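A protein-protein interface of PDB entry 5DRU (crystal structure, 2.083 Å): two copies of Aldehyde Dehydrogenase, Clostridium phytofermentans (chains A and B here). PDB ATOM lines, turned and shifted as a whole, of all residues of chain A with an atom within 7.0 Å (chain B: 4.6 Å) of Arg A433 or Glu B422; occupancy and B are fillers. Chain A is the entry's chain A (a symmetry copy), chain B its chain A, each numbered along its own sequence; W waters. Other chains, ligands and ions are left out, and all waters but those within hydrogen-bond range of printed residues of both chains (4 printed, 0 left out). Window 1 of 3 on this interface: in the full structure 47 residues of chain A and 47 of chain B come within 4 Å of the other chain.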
ATOM      1  N   VAL A 105      11.950 -24.219 -30.188  1.00  0.00           N
ATOM      2  CA  VAL A 105      12.653 -23.074 -29.625  1.00  0.00           C
ATOM      3  C   VAL A 105      14.137 -23.386 -29.670  1.00  0.00           C
ATOM      4  O   VAL A 105      14.579 -24.361 -29.047  1.00  0.00           O
ATOM      5  CB  VAL A 105      12.242 -22.763 -28.176  1.00  0.00           C
ATOM      6  CG1 VAL A 105      13.098 -21.628 -27.563  1.00  0.00           C
ATOM      7  CG2 VAL A 105      10.699 -22.412 -28.073  1.00  0.00           C
ATOM      8  N   GLU A 106      14.870 -22.514 -30.354  1.00  0.00           N
ATOM      9  CA  GLU A 106      16.299 -22.617 -30.550  1.00  0.00           C
ATOM     10  C   GLU A 106      17.065 -21.457 -29.924  1.00  0.00           C
ATOM     11  O   GLU A 106      16.504 -20.414 -29.569  1.00  0.00           O
ATOM     12  CB  GLU A 106      16.629 -22.652 -32.033  1.00  0.00           C
ATOM     13  CG  GLU A 106      16.037 -23.840 -32.713  1.00  0.00           C
ATOM     14  CD  GLU A 106      16.949 -25.015 -32.681  1.00  0.00           C
ATOM     15  OE1 GLU A 106      17.961 -24.986 -31.876  1.00  0.00           O
ATOM     16  OE2 GLU A 106      16.656 -25.939 -33.486  1.00  0.00           O
ATOM     17  N   MET A 107      18.377 -21.682 -29.848  1.00  0.00           N
ATOM     18  CA  MET A 107      19.357 -20.760 -29.295  1.00  0.00           C
ATOM     19  C   MET A 107      20.203 -20.320 -30.474  1.00  0.00           C
ATOM     20  O   MET A 107      21.053 -21.093 -30.949  1.00  0.00           O
ATOM     21  CB  MET A 107      20.209 -21.458 -28.242  1.00  0.00           C
ATOM     22  CG  MET A 107      19.510 -21.795 -26.963  1.00  0.00           C
ATOM     23  SD  MET A 107      20.576 -22.740 -25.868  1.00  0.00           S
ATOM     24  CE  MET A 107      19.356 -23.182 -24.586  1.00  0.00           C
ATOM     25  N   GLY A 108      19.942 -19.112 -30.971  1.00  0.00           N
ATOM     26  CA  GLY A 108      20.620 -18.575 -32.124  1.00  0.00           C
ATOM     27  C   GLY A 108      21.729 -17.656 -31.712  1.00  0.00           C
ATOM     28  O   GLY A 108      21.771 -17.191 -30.579  1.00  0.00           O
ATOM     29  N   PHE A 110      24.062 -14.402 -30.990  1.00  0.00           N
ATOM     30  CA  PHE A 110      23.980 -12.930 -30.935  1.00  0.00           C
ATOM     31  C   PHE A 110      24.698 -12.223 -32.079  1.00  0.00           C
ATOM     32  O   PHE A 110      24.099 -11.369 -32.775  1.00  0.00           O
ATOM     33  CB  PHE A 110      24.570 -12.421 -29.633  1.00  0.00           C
ATOM     34  CG  PHE A 110      23.573 -12.128 -28.617  1.00  0.00           C
ATOM     35  CD1 PHE A 110      22.877 -10.908 -28.611  1.00  0.00           C
ATOM     36  CD2 PHE A 110      23.328 -13.049 -27.645  1.00  0.00           C
ATOM     37  CE1 PHE A 110      21.940 -10.634 -27.625  1.00  0.00           C
ATOM     38  CE2 PHE A 110      22.343 -12.796 -26.656  1.00  0.00           C
ATOM     39  CZ  PHE A 110      21.685 -11.591 -26.643  1.00  0.00           C
ATOM     40  N   ARG A 214      22.518  -5.013 -24.115  1.00  0.00           N
ATOM     41  CA  ARG A 214      22.403  -5.968 -23.043  1.00  0.00           C
ATOM     42  C   ARG A 214      23.772  -6.213 -22.442  1.00  0.00           C
ATOM     43  O   ARG A 214      24.715  -6.503 -23.165  1.00  0.00           O
ATOM     44  CB  ARG A 214      21.855  -7.292 -23.520  1.00  0.00           C
ATOM     45  CG  ARG A 214      21.644  -8.193 -22.348  1.00  0.00           C
ATOM     46  CD  ARG A 214      20.935  -9.401 -22.685  1.00  0.00           C
ATOM     47  NE  ARG A 214      21.075 -10.347 -21.572  1.00  0.00           N
ATOM     48  CZ  ARG A 214      20.664 -11.601 -21.659  1.00  0.00           C
ATOM     49  NH1 ARG A 214      20.177 -11.990 -22.792  1.00  0.00           N
ATOM     50  NH2 ARG A 214      20.841 -12.478 -20.663  1.00  0.00           N
ATOM     51  N   GLU A 422      22.079 -14.230 -14.687  1.00  0.00           N
ATOM     52  CA  GLU A 422      22.226 -15.410 -15.521  1.00  0.00           C
ATOM     53  C   GLU A 422      23.017 -16.508 -14.775  1.00  0.00           C
ATOM     54  O   GLU A 422      23.024 -17.663 -15.173  1.00  0.00           O
ATOM     55  CB  GLU A 422      22.903 -15.025 -16.847  1.00  0.00           C
ATOM     56  CG  GLU A 422      22.078 -14.026 -17.732  1.00  0.00           C
ATOM     57  CD  GLU A 422      22.326 -12.502 -17.432  1.00  0.00           C
ATOM     58  OE1 GLU A 422      23.087 -12.165 -16.488  1.00  0.00           O
ATOM     59  OE2 GLU A 422      21.785 -11.614 -18.165  1.00  0.00           O
ATOM     60  N   ALA A 427      27.747 -21.315 -22.849  1.00  0.00           N
ATOM     61  CA  ALA A 427      27.352 -21.061 -24.229  1.00  0.00           C
ATOM     62  C   ALA A 427      25.865 -20.623 -24.337  1.00  0.00           C
ATOM     63  O   ALA A 427      25.540 -19.620 -24.986  1.00  0.00           O
ATOM     64  CB  ALA A 427      27.600 -22.306 -25.072  1.00  0.00           C
ATOM     65  N   SER A 428      24.983 -21.347 -23.680  1.00  0.00           N
ATOM     66  CA  SER A 428      23.553 -21.039 -23.763  1.00  0.00           C
ATOM     67  C   SER A 428      23.204 -19.607 -23.332  1.00  0.00           C
ATOM     68  O   SER A 428      22.319 -19.025 -23.927  1.00  0.00           O
ATOM     69  CB  SER A 428      22.703 -22.029 -22.963  1.00  0.00           C
ATOM     70  OG  SER A 428      23.096 -22.165 -21.620  1.00  0.00           O
ATOM     71  N   THR A 429      23.854 -19.075 -22.303  1.00  0.00           N
ATOM     72  CA  THR A 429      23.725 -17.664 -21.904  1.00  0.00           C
ATOM     73  C   THR A 429      23.885 -16.702 -23.085  1.00  0.00           C
ATOM     74  O   THR A 429      23.155 -15.720 -23.242  1.00  0.00           O
ATOM     75  CB  THR A 429      24.796 -17.302 -20.823  1.00  0.00           C
ATOM     76  OG1 THR A 429      24.972 -18.404 -19.920  1.00  0.00           O
ATOM     77  CG2 THR A 429      24.399 -16.057 -20.050  1.00  0.00           C
ATOM     78  N   PHE A 430      24.843 -16.988 -23.950  1.00  0.00           N
ATOM     79  CA  PHE A 430      25.221 -16.033 -24.973  1.00  0.00           C
ATOM     80  C   PHE A 430      24.507 -16.322 -26.295  1.00  0.00           C
ATOM     81  O   PHE A 430      25.091 -16.188 -27.390  1.00  0.00           O
ATOM     82  CB  PHE A 430      26.738 -16.057 -25.163  1.00  0.00           C
ATOM     83  CG  PHE A 430      27.525 -15.953 -23.868  1.00  0.00           C
ATOM     84  CD1 PHE A 430      27.479 -14.789 -23.108  1.00  0.00           C
ATOM     85  CD2 PHE A 430      28.347 -16.992 -23.453  1.00  0.00           C
ATOM     86  CE1 PHE A 430      28.239 -14.661 -21.956  1.00  0.00           C
ATOM     87  CE2 PHE A 430      29.106 -16.883 -22.273  1.00  0.00           C
ATOM     88  CZ  PHE A 430      29.047 -15.725 -21.522  1.00  0.00           C
ATOM     89  N   THR A 431      23.251 -16.739 -26.188  1.00  0.00           N
ATOM     90  CA  THR A 431      22.402 -16.898 -27.371  1.00  0.00           C
ATOM     91  C   THR A 431      21.091 -16.159 -27.238  1.00  0.00           C
ATOM     92  O   THR A 431      20.650 -15.825 -26.132  1.00  0.00           O
ATOM     93  CB  THR A 431      22.101 -18.396 -27.675  1.00  0.00           C
ATOM     94  OG1 THR A 431      21.345 -19.030 -26.609  1.00  0.00           O
ATOM     95  CG2 THR A 431      23.408 -19.144 -27.899  1.00  0.00           C
ATOM     96  N   LYS A 432      20.493 -15.915 -28.401  1.00  0.00           N
ATOM     97  CA  LYS A 432      19.125 -15.413 -28.513  1.00  0.00           C
ATOM     98  C   LYS A 432      18.123 -16.557 -28.741  1.00  0.00           C
ATOM     99  O   LYS A 432      18.367 -17.477 -29.522  1.00  0.00           O
ATOM    100  CB  LYS A 432      19.007 -14.415 -29.660  1.00  0.00           C
ATOM    101  CG  LYS A 432      20.059 -13.321 -29.625  1.00  0.00           C
ATOM    102  CD  LYS A 432      19.768 -12.107 -30.519  1.00  0.00           C
ATOM    103  CE  LYS A 432      18.462 -11.424 -30.129  1.00  0.00           C
ATOM    104  NZ  LYS A 432      18.184 -10.324 -31.084  1.00  0.00           N
ATOM    105  N   ARG A 433      16.983 -16.484 -28.073  1.00  0.00           N
ATOM    106  CA  ARG A 433      15.938 -17.505 -28.222  1.00  0.00           C
ATOM    107  C   ARG A 433      15.100 -17.184 -29.459  1.00  0.00           C
ATOM    108  O   ARG A 433      14.823 -16.007 -29.788  1.00  0.00           O
ATOM    109  CB  ARG A 433      15.091 -17.590 -26.965  1.00  0.00           C
ATOM    110  CG  ARG A 433      15.910 -17.640 -25.676  1.00  0.00           C
ATOM    111  CD  ARG A 433      16.207 -19.118 -25.289  1.00  0.00           C
ATOM    112  NE  ARG A 433      17.241 -19.320 -24.251  1.00  0.00           N
ATOM    113  CZ  ARG A 433      18.548 -19.109 -24.427  1.00  0.00           C
ATOM    114  NH1 ARG A 433      18.959 -18.613 -25.592  1.00  0.00           N
ATOM    115  NH2 ARG A 433      19.450 -19.362 -23.421  1.00  0.00           N
ATOM    116  N   ARG A 434      14.750 -18.257 -30.160  1.00  0.00           N
ATOM    117  CA  ARG A 434      14.063 -18.195 -31.445  1.00  0.00           C
ATOM    118  C   ARG A 434      12.938 -19.210 -31.418  1.00  0.00           C
ATOM    119  O   ARG A 434      13.176 -20.391 -31.240  1.00  0.00           O
ATOM    120  CB  ARG A 434      15.008 -18.497 -32.603  1.00  0.00           C
ATOM    121  CG  ARG A 434      16.149 -17.532 -32.701  1.00  0.00           C
ATOM    122  CD  ARG A 434      16.807 -17.630 -34.054  1.00  0.00           C
ATOM    123  NE  ARG A 434      15.843 -17.569 -35.145  1.00  0.00           N
ATOM    124  CZ  ARG A 434      16.090 -18.021 -36.370  1.00  0.00           C
ATOM    125  NH1 ARG A 434      17.278 -18.552 -36.666  1.00  0.00           N
ATOM    126  NH2 ARG A 434      15.160 -17.960 -37.303  1.00  0.00           N
ATOM    127  N   ARG A 435      11.709 -18.747 -31.535  1.00  0.00           N
ATOM    128  CA  ARG A 435      10.584 -19.678 -31.604  1.00  0.00           C
ATOM    129  C   ARG A 435      10.189 -19.846 -33.054  1.00  0.00           C
ATOM    130  O   ARG A 435      10.055 -18.887 -33.796  1.00  0.00           O
ATOM    131  CB  ARG A 435       9.378 -19.210 -30.784  1.00  0.00           C
ATOM    132  CG  ARG A 435       8.192 -20.218 -30.822  1.00  0.00           C
ATOM    133  CD  ARG A 435       6.905 -19.731 -30.106  1.00  0.00           C
ATOM    134  NE  ARG A 435       7.083 -19.685 -28.646  1.00  0.00           N
ATOM    135  CZ  ARG A 435       6.084 -19.578 -27.776  1.00  0.00           C
ATOM    136  NH1 ARG A 435       4.801 -19.507 -28.192  1.00  0.00           N
ATOM    137  NH2 ARG A 435       6.381 -19.510 -26.490  1.00  0.00           N
ATOM    138  N   ARG B 214      19.823  -4.412 -15.336  1.00  0.00           N
ATOM    139  CA  ARG B 214      19.481  -5.293 -16.423  1.00  0.00           C
ATOM    140  C   ARG B 214      18.159  -4.861 -17.023  1.00  0.00           C
ATOM    141  O   ARG B 214      17.188  -4.687 -16.300  1.00  0.00           O
ATOM    142  CB  ARG B 214      19.345  -6.727 -15.968  1.00  0.00           C
ATOM    143  CG  ARG B 214      19.114  -7.605 -17.153  1.00  0.00           C
ATOM    144  CD  ARG B 214      19.173  -9.009 -16.836  1.00  0.00           C
ATOM    145  NE  ARG B 214      18.611  -9.763 -17.963  1.00  0.00           N
ATOM    146  CZ  ARG B 214      18.387 -11.065 -17.896  1.00  0.00           C
ATOM    147  NH1 ARG B 214      18.631 -11.653 -16.770  1.00  0.00           N
ATOM    148  NH2 ARG B 214      17.824 -11.743 -18.904  1.00  0.00           N
ATOM    149  N   GLY B 215      18.139  -4.712 -18.341  1.00  0.00           N
ATOM    150  CA  GLY B 215      16.956  -4.370 -19.074  1.00  0.00           C
ATOM    151  C   GLY B 215      16.602  -5.528 -19.991  1.00  0.00           C
ATOM    152  O   GLY B 215      17.448  -6.080 -20.681  1.00  0.00           O
ATOM    153  N   ILE B 216      15.345  -5.922 -19.951  1.00  0.00           N
ATOM    154  CA  ILE B 216      14.801  -6.919 -20.887  1.00  0.00           C
ATOM    155  C   ILE B 216      14.013  -6.140 -21.893  1.00  0.00           C
ATOM    156  O   ILE B 216      13.071  -5.432 -21.544  1.00  0.00           O
ATOM    157  CB  ILE B 216      13.939  -7.968 -20.175  1.00  0.00           C
ATOM    158  CG1 ILE B 216      14.836  -8.878 -19.341  1.00  0.00           C
ATOM    159  CG2 ILE B 216      13.201  -8.791 -21.155  1.00  0.00           C
ATOM    160  CD1 ILE B 216      14.150  -9.538 -18.241  1.00  0.00           C
ATOM    161  N   GLY B 217      14.456  -6.217 -23.140  1.00  0.00           N
ATOM    162  CA  GLY B 217      14.127  -5.203 -24.112  1.00  0.00           C
ATOM    163  C   GLY B 217      13.286  -5.755 -25.240  1.00  0.00           C
ATOM    164  O   GLY B 217      13.749  -6.545 -26.057  1.00  0.00           O
ATOM    165  N   ALA B 392      13.221 -13.624 -33.626  1.00  0.00           N
ATOM    166  CA  ALA B 392      12.767 -14.224 -32.383  1.00  0.00           C
ATOM    167  C   ALA B 392      11.569 -15.115 -32.590  1.00  0.00           C
ATOM    168  O   ALA B 392      11.257 -15.995 -31.766  1.00  0.00           O
ATOM    169  CB  ALA B 392      12.441 -13.157 -31.388  1.00  0.00           C
ATOM    170  N   ALA B 417      11.046 -10.319 -26.125  1.00  0.00           N
ATOM    171  CA  ALA B 417      12.313  -9.547 -25.939  1.00  0.00           C
ATOM    172  C   ALA B 417      13.320  -9.742 -27.067  1.00  0.00           C
ATOM    173  O   ALA B 417      14.371 -10.346 -26.856  1.00  0.00           O
ATOM    174  CB  ALA B 417      12.958  -9.906 -24.606  1.00  0.00           C
ATOM    175  N   THR B 420      17.252  -7.899 -26.578  1.00  0.00           N
ATOM    176  CA  THR B 420      18.158  -8.328 -25.530  1.00  0.00           C
ATOM    177  C   THR B 420      18.218  -9.834 -25.461  1.00  0.00           C
ATOM    178  O   THR B 420      19.030 -10.392 -24.724  1.00  0.00           O
ATOM    179  CB  THR B 420      17.725  -7.755 -24.163  1.00  0.00           C
ATOM    180  OG1 THR B 420      16.391  -8.164 -23.866  1.00  0.00           O
ATOM    181  CG2 THR B 420      17.787  -6.256 -24.184  1.00  0.00           C
ATOM    182  N   GLY B 421      17.318 -10.490 -26.206  1.00  0.00           N
ATOM    183  CA  GLY B 421      17.491 -11.878 -26.600  1.00  0.00           C
ATOM    184  C   GLY B 421      16.782 -12.987 -25.853  1.00  0.00           C
ATOM    185  O   GLY B 421      16.960 -14.168 -26.178  1.00  0.00           O
ATOM    186  N   GLU B 422      15.932 -12.623 -24.900  1.00  0.00           N
ATOM    187  CA  GLU B 422      15.247 -13.609 -24.083  1.00  0.00           C
ATOM    188  C   GLU B 422      14.037 -14.199 -24.842  1.00  0.00           C
ATOM    189  O   GLU B 422      13.489 -15.222 -24.461  1.00  0.00           O
ATOM    190  CB  GLU B 422      14.824 -12.972 -22.750  1.00  0.00           C
ATOM    191  CG  GLU B 422      16.017 -12.488 -21.853  1.00  0.00           C
ATOM    192  CD  GLU B 422      16.512 -11.021 -22.130  1.00  0.00           C
ATOM    193  OE1 GLU B 422      16.001 -10.353 -23.066  1.00  0.00           O
ATOM    194  OE2 GLU B 422      17.404 -10.500 -21.386  1.00  0.00           O
ATOM    195  N   GLY B 423      13.690 -13.592 -25.969  1.00  0.00           N
ATOM    196  CA  GLY B 423      12.592 -14.099 -26.781  1.00  0.00           C
ATOM    197  C   GLY B 423      11.234 -13.874 -26.114  1.00  0.00           C
ATOM    198  O   GLY B 423      10.945 -12.790 -25.597  1.00  0.00           O
ATOM    199  N   LEU B 424      10.395 -14.888 -26.136  1.00  0.00           N
ATOM    200  CA  LEU B 424       9.056 -14.752 -25.607  1.00  0.00           C
ATOM    201  C   LEU B 424       9.113 -14.861 -24.069  1.00  0.00           C
ATOM    202  O   LEU B 424       9.379 -15.949 -23.548  1.00  0.00           O
ATOM    203  CB  LEU B 424       8.144 -15.824 -26.232  1.00  0.00           C
ATOM    204  CG  LEU B 424       7.516 -15.413 -27.595  1.00  0.00           C
ATOM    205  CD1 LEU B 424       8.428 -15.613 -28.839  1.00  0.00           C
ATOM    206  CD2 LEU B 424       6.306 -16.145 -27.809  1.00  0.00           C
ATOM    207  N   THR B 429      12.069 -16.186 -17.351  1.00  0.00           N
ATOM    208  CA  THR B 429      12.844 -14.993 -17.729  1.00  0.00           C
ATOM    209  C   THR B 429      13.148 -14.085 -16.534  1.00  0.00           C
ATOM    210  O   THR B 429      14.253 -13.562 -16.365  1.00  0.00           O
ATOM    211  CB  THR B 429      12.071 -14.156 -18.800  1.00  0.00           C
ATOM    212  OG1 THR B 429      11.403 -15.034 -19.719  1.00  0.00           O
ATOM    213  CG2 THR B 429      13.007 -13.231 -19.557  1.00  0.00           C
HETATM  214  O   HOH W   1      21.757  -9.018 -18.925  1.00  0.00           O
HETATM  215  O   HOH W   2      15.457 -13.255 -29.165  1.00  0.00           O
HETATM  216  O   HOH W   3      12.060 -16.101 -29.355  1.00  0.00           O
HETATM  217  O   HOH W   4      18.641  -8.231 -20.588  1.00  0.00           O
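Printed residues of chain B that touch a printed residue of chain A: Arg B214, Ala B392, Thr B420, Gly B421, Glu B422 and Leu B424.
Hydrophobic or aromatic side chains of chain B that line the printed part of chain A: Leu B424.
Printed residues of chain A that touch a printed residue of chain B: Phe A110, Arg A214, Glu A422, Lys A432, Arg A433, Arg A434 and Arg A435.
Among the printed residues, Asp or Glu carboxylates within 4 Å of a Lys or Arg side-chain nitrogen of the other chain: Arg A214 with Glu B422 (3.4 Å) and Glu A422 with Arg B214 (3.4 Å).
Phe A110 touches Thr B420 (CZ to O, 3.5 Å).
Arg B214 touches Arg A214 (NH2 to NH2, 3.6 Å).
O of Gly B421 touches CA of Lys A432 (3.4 Å).
Arg A433 touches Ala B392.
Arg A433 touches Glu B422.
Arg A434 touches Ala B392.
CZ of Arg A435 touches CD2 of Leu B424, 3.4 Å away.
NH1 of Arg A214 lies within salt-bridge range of OE2 of Glu B422 (3.4 Å).
The backbone carbonyl oxygen (O) of Gly B421 is in hydrogen-bond range of the backbone NH (N) of Arg A433 (3.0 Å).
The guanidinium group (NH1) of Arg B214 lies within salt-bridge range of the side-chain carboxylate (OE2) of Glu A422 (3.4 Å).
O of Thr B420 sits at hydrogen-bond distance from NH1 of Arg A214.
The backbone NH (N) of Arg A435 is in hydrogen-bond range of the backbone carbonyl oxygen (O) of Ala B392 (2.8 Å).
N of Gly A108 is in hydrogen-bond range of O of Lys A432, 2.7 Å away.
The backbone NH of Arg A434 lies within hydrogen-bond range of the backbone carbonyl oxygen of Glu A106 (2.8 Å).
The backbone carbonyl oxygen (O) of Ser A428 lies within hydrogen-bond range of the guanidinium group (NH2) of Arg A433, 2.9 Å away.
The guanidinium group of Arg B214 is in salt-bridge range of the side-chain carboxylate of Glu B422, at 2.8 Å.
The side-chain hydroxyl (OG1) of Thr B420 sits at hydrogen-bond distance from the backbone NH (N) of Gly B217.
The backbone carbonyl oxygen of Ala B417 lies within hydrogen-bond range of the backbone NH of Glu B422 (3.4 Å).
Arg B214 touches its own counterpart, Arg A214.
Arg A214 touches Glu B422, and with the chains exchanged Glu A422 touches Arg B214.
Positions printed for both chains: 214, 422 and 429.
Water W4 lies within hydrogen-bond range of O of Gly B215 (2.5 Å), OE2 of Glu B422 (2.7 Å), NE of Arg B214 (3.0 Å) and NE of Arg A214 (3.4 Å).
Water W3 lies within hydrogen-bond range of the backbone carbonyl oxygen (O) of Ala B392 (2.5 Å), the backbone carbonyl oxygen (O) of Arg A433 (2.8 Å) and the backbone NH (N) of Arg A435 (3.4 Å).
Water W1 lies within hydrogen-bond range of OE2 of Glu A422 (2.7 Å), NE of Arg A214 (3.0 Å) and NE of Arg B214 (3.4 Å).
Water W2 bridges O of Arg A433 (2.9 Å) and O of Gly B421 (3.5 Å).
Printed residues of chain B within 4 Å of Phe A110: Thr B420 (3.5 Å).
Of the printed residues of chain B, Arg A214 touches Arg B214, Thr B420 and Glu B422.
Of the printed residues of chain B, Glu A422 touches Arg B214.
Thr A429 touches none of the printed residues of chain B.
Of chain B, only Ala B392, Gly B421 and Glu B422 come within 4 Å of Arg A433.
Of the printed residues of chain B, Arg A435 touches Ala B392 and Leu B424.
Of the printed residues of chain A, Gly B421 touches Lys A432 and Arg A433.
Of chain A, only Arg A214 and Arg A433 come within 4 Å of Glu B422.
Of the printed residues of chain A, Leu B424 touches Arg A435.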
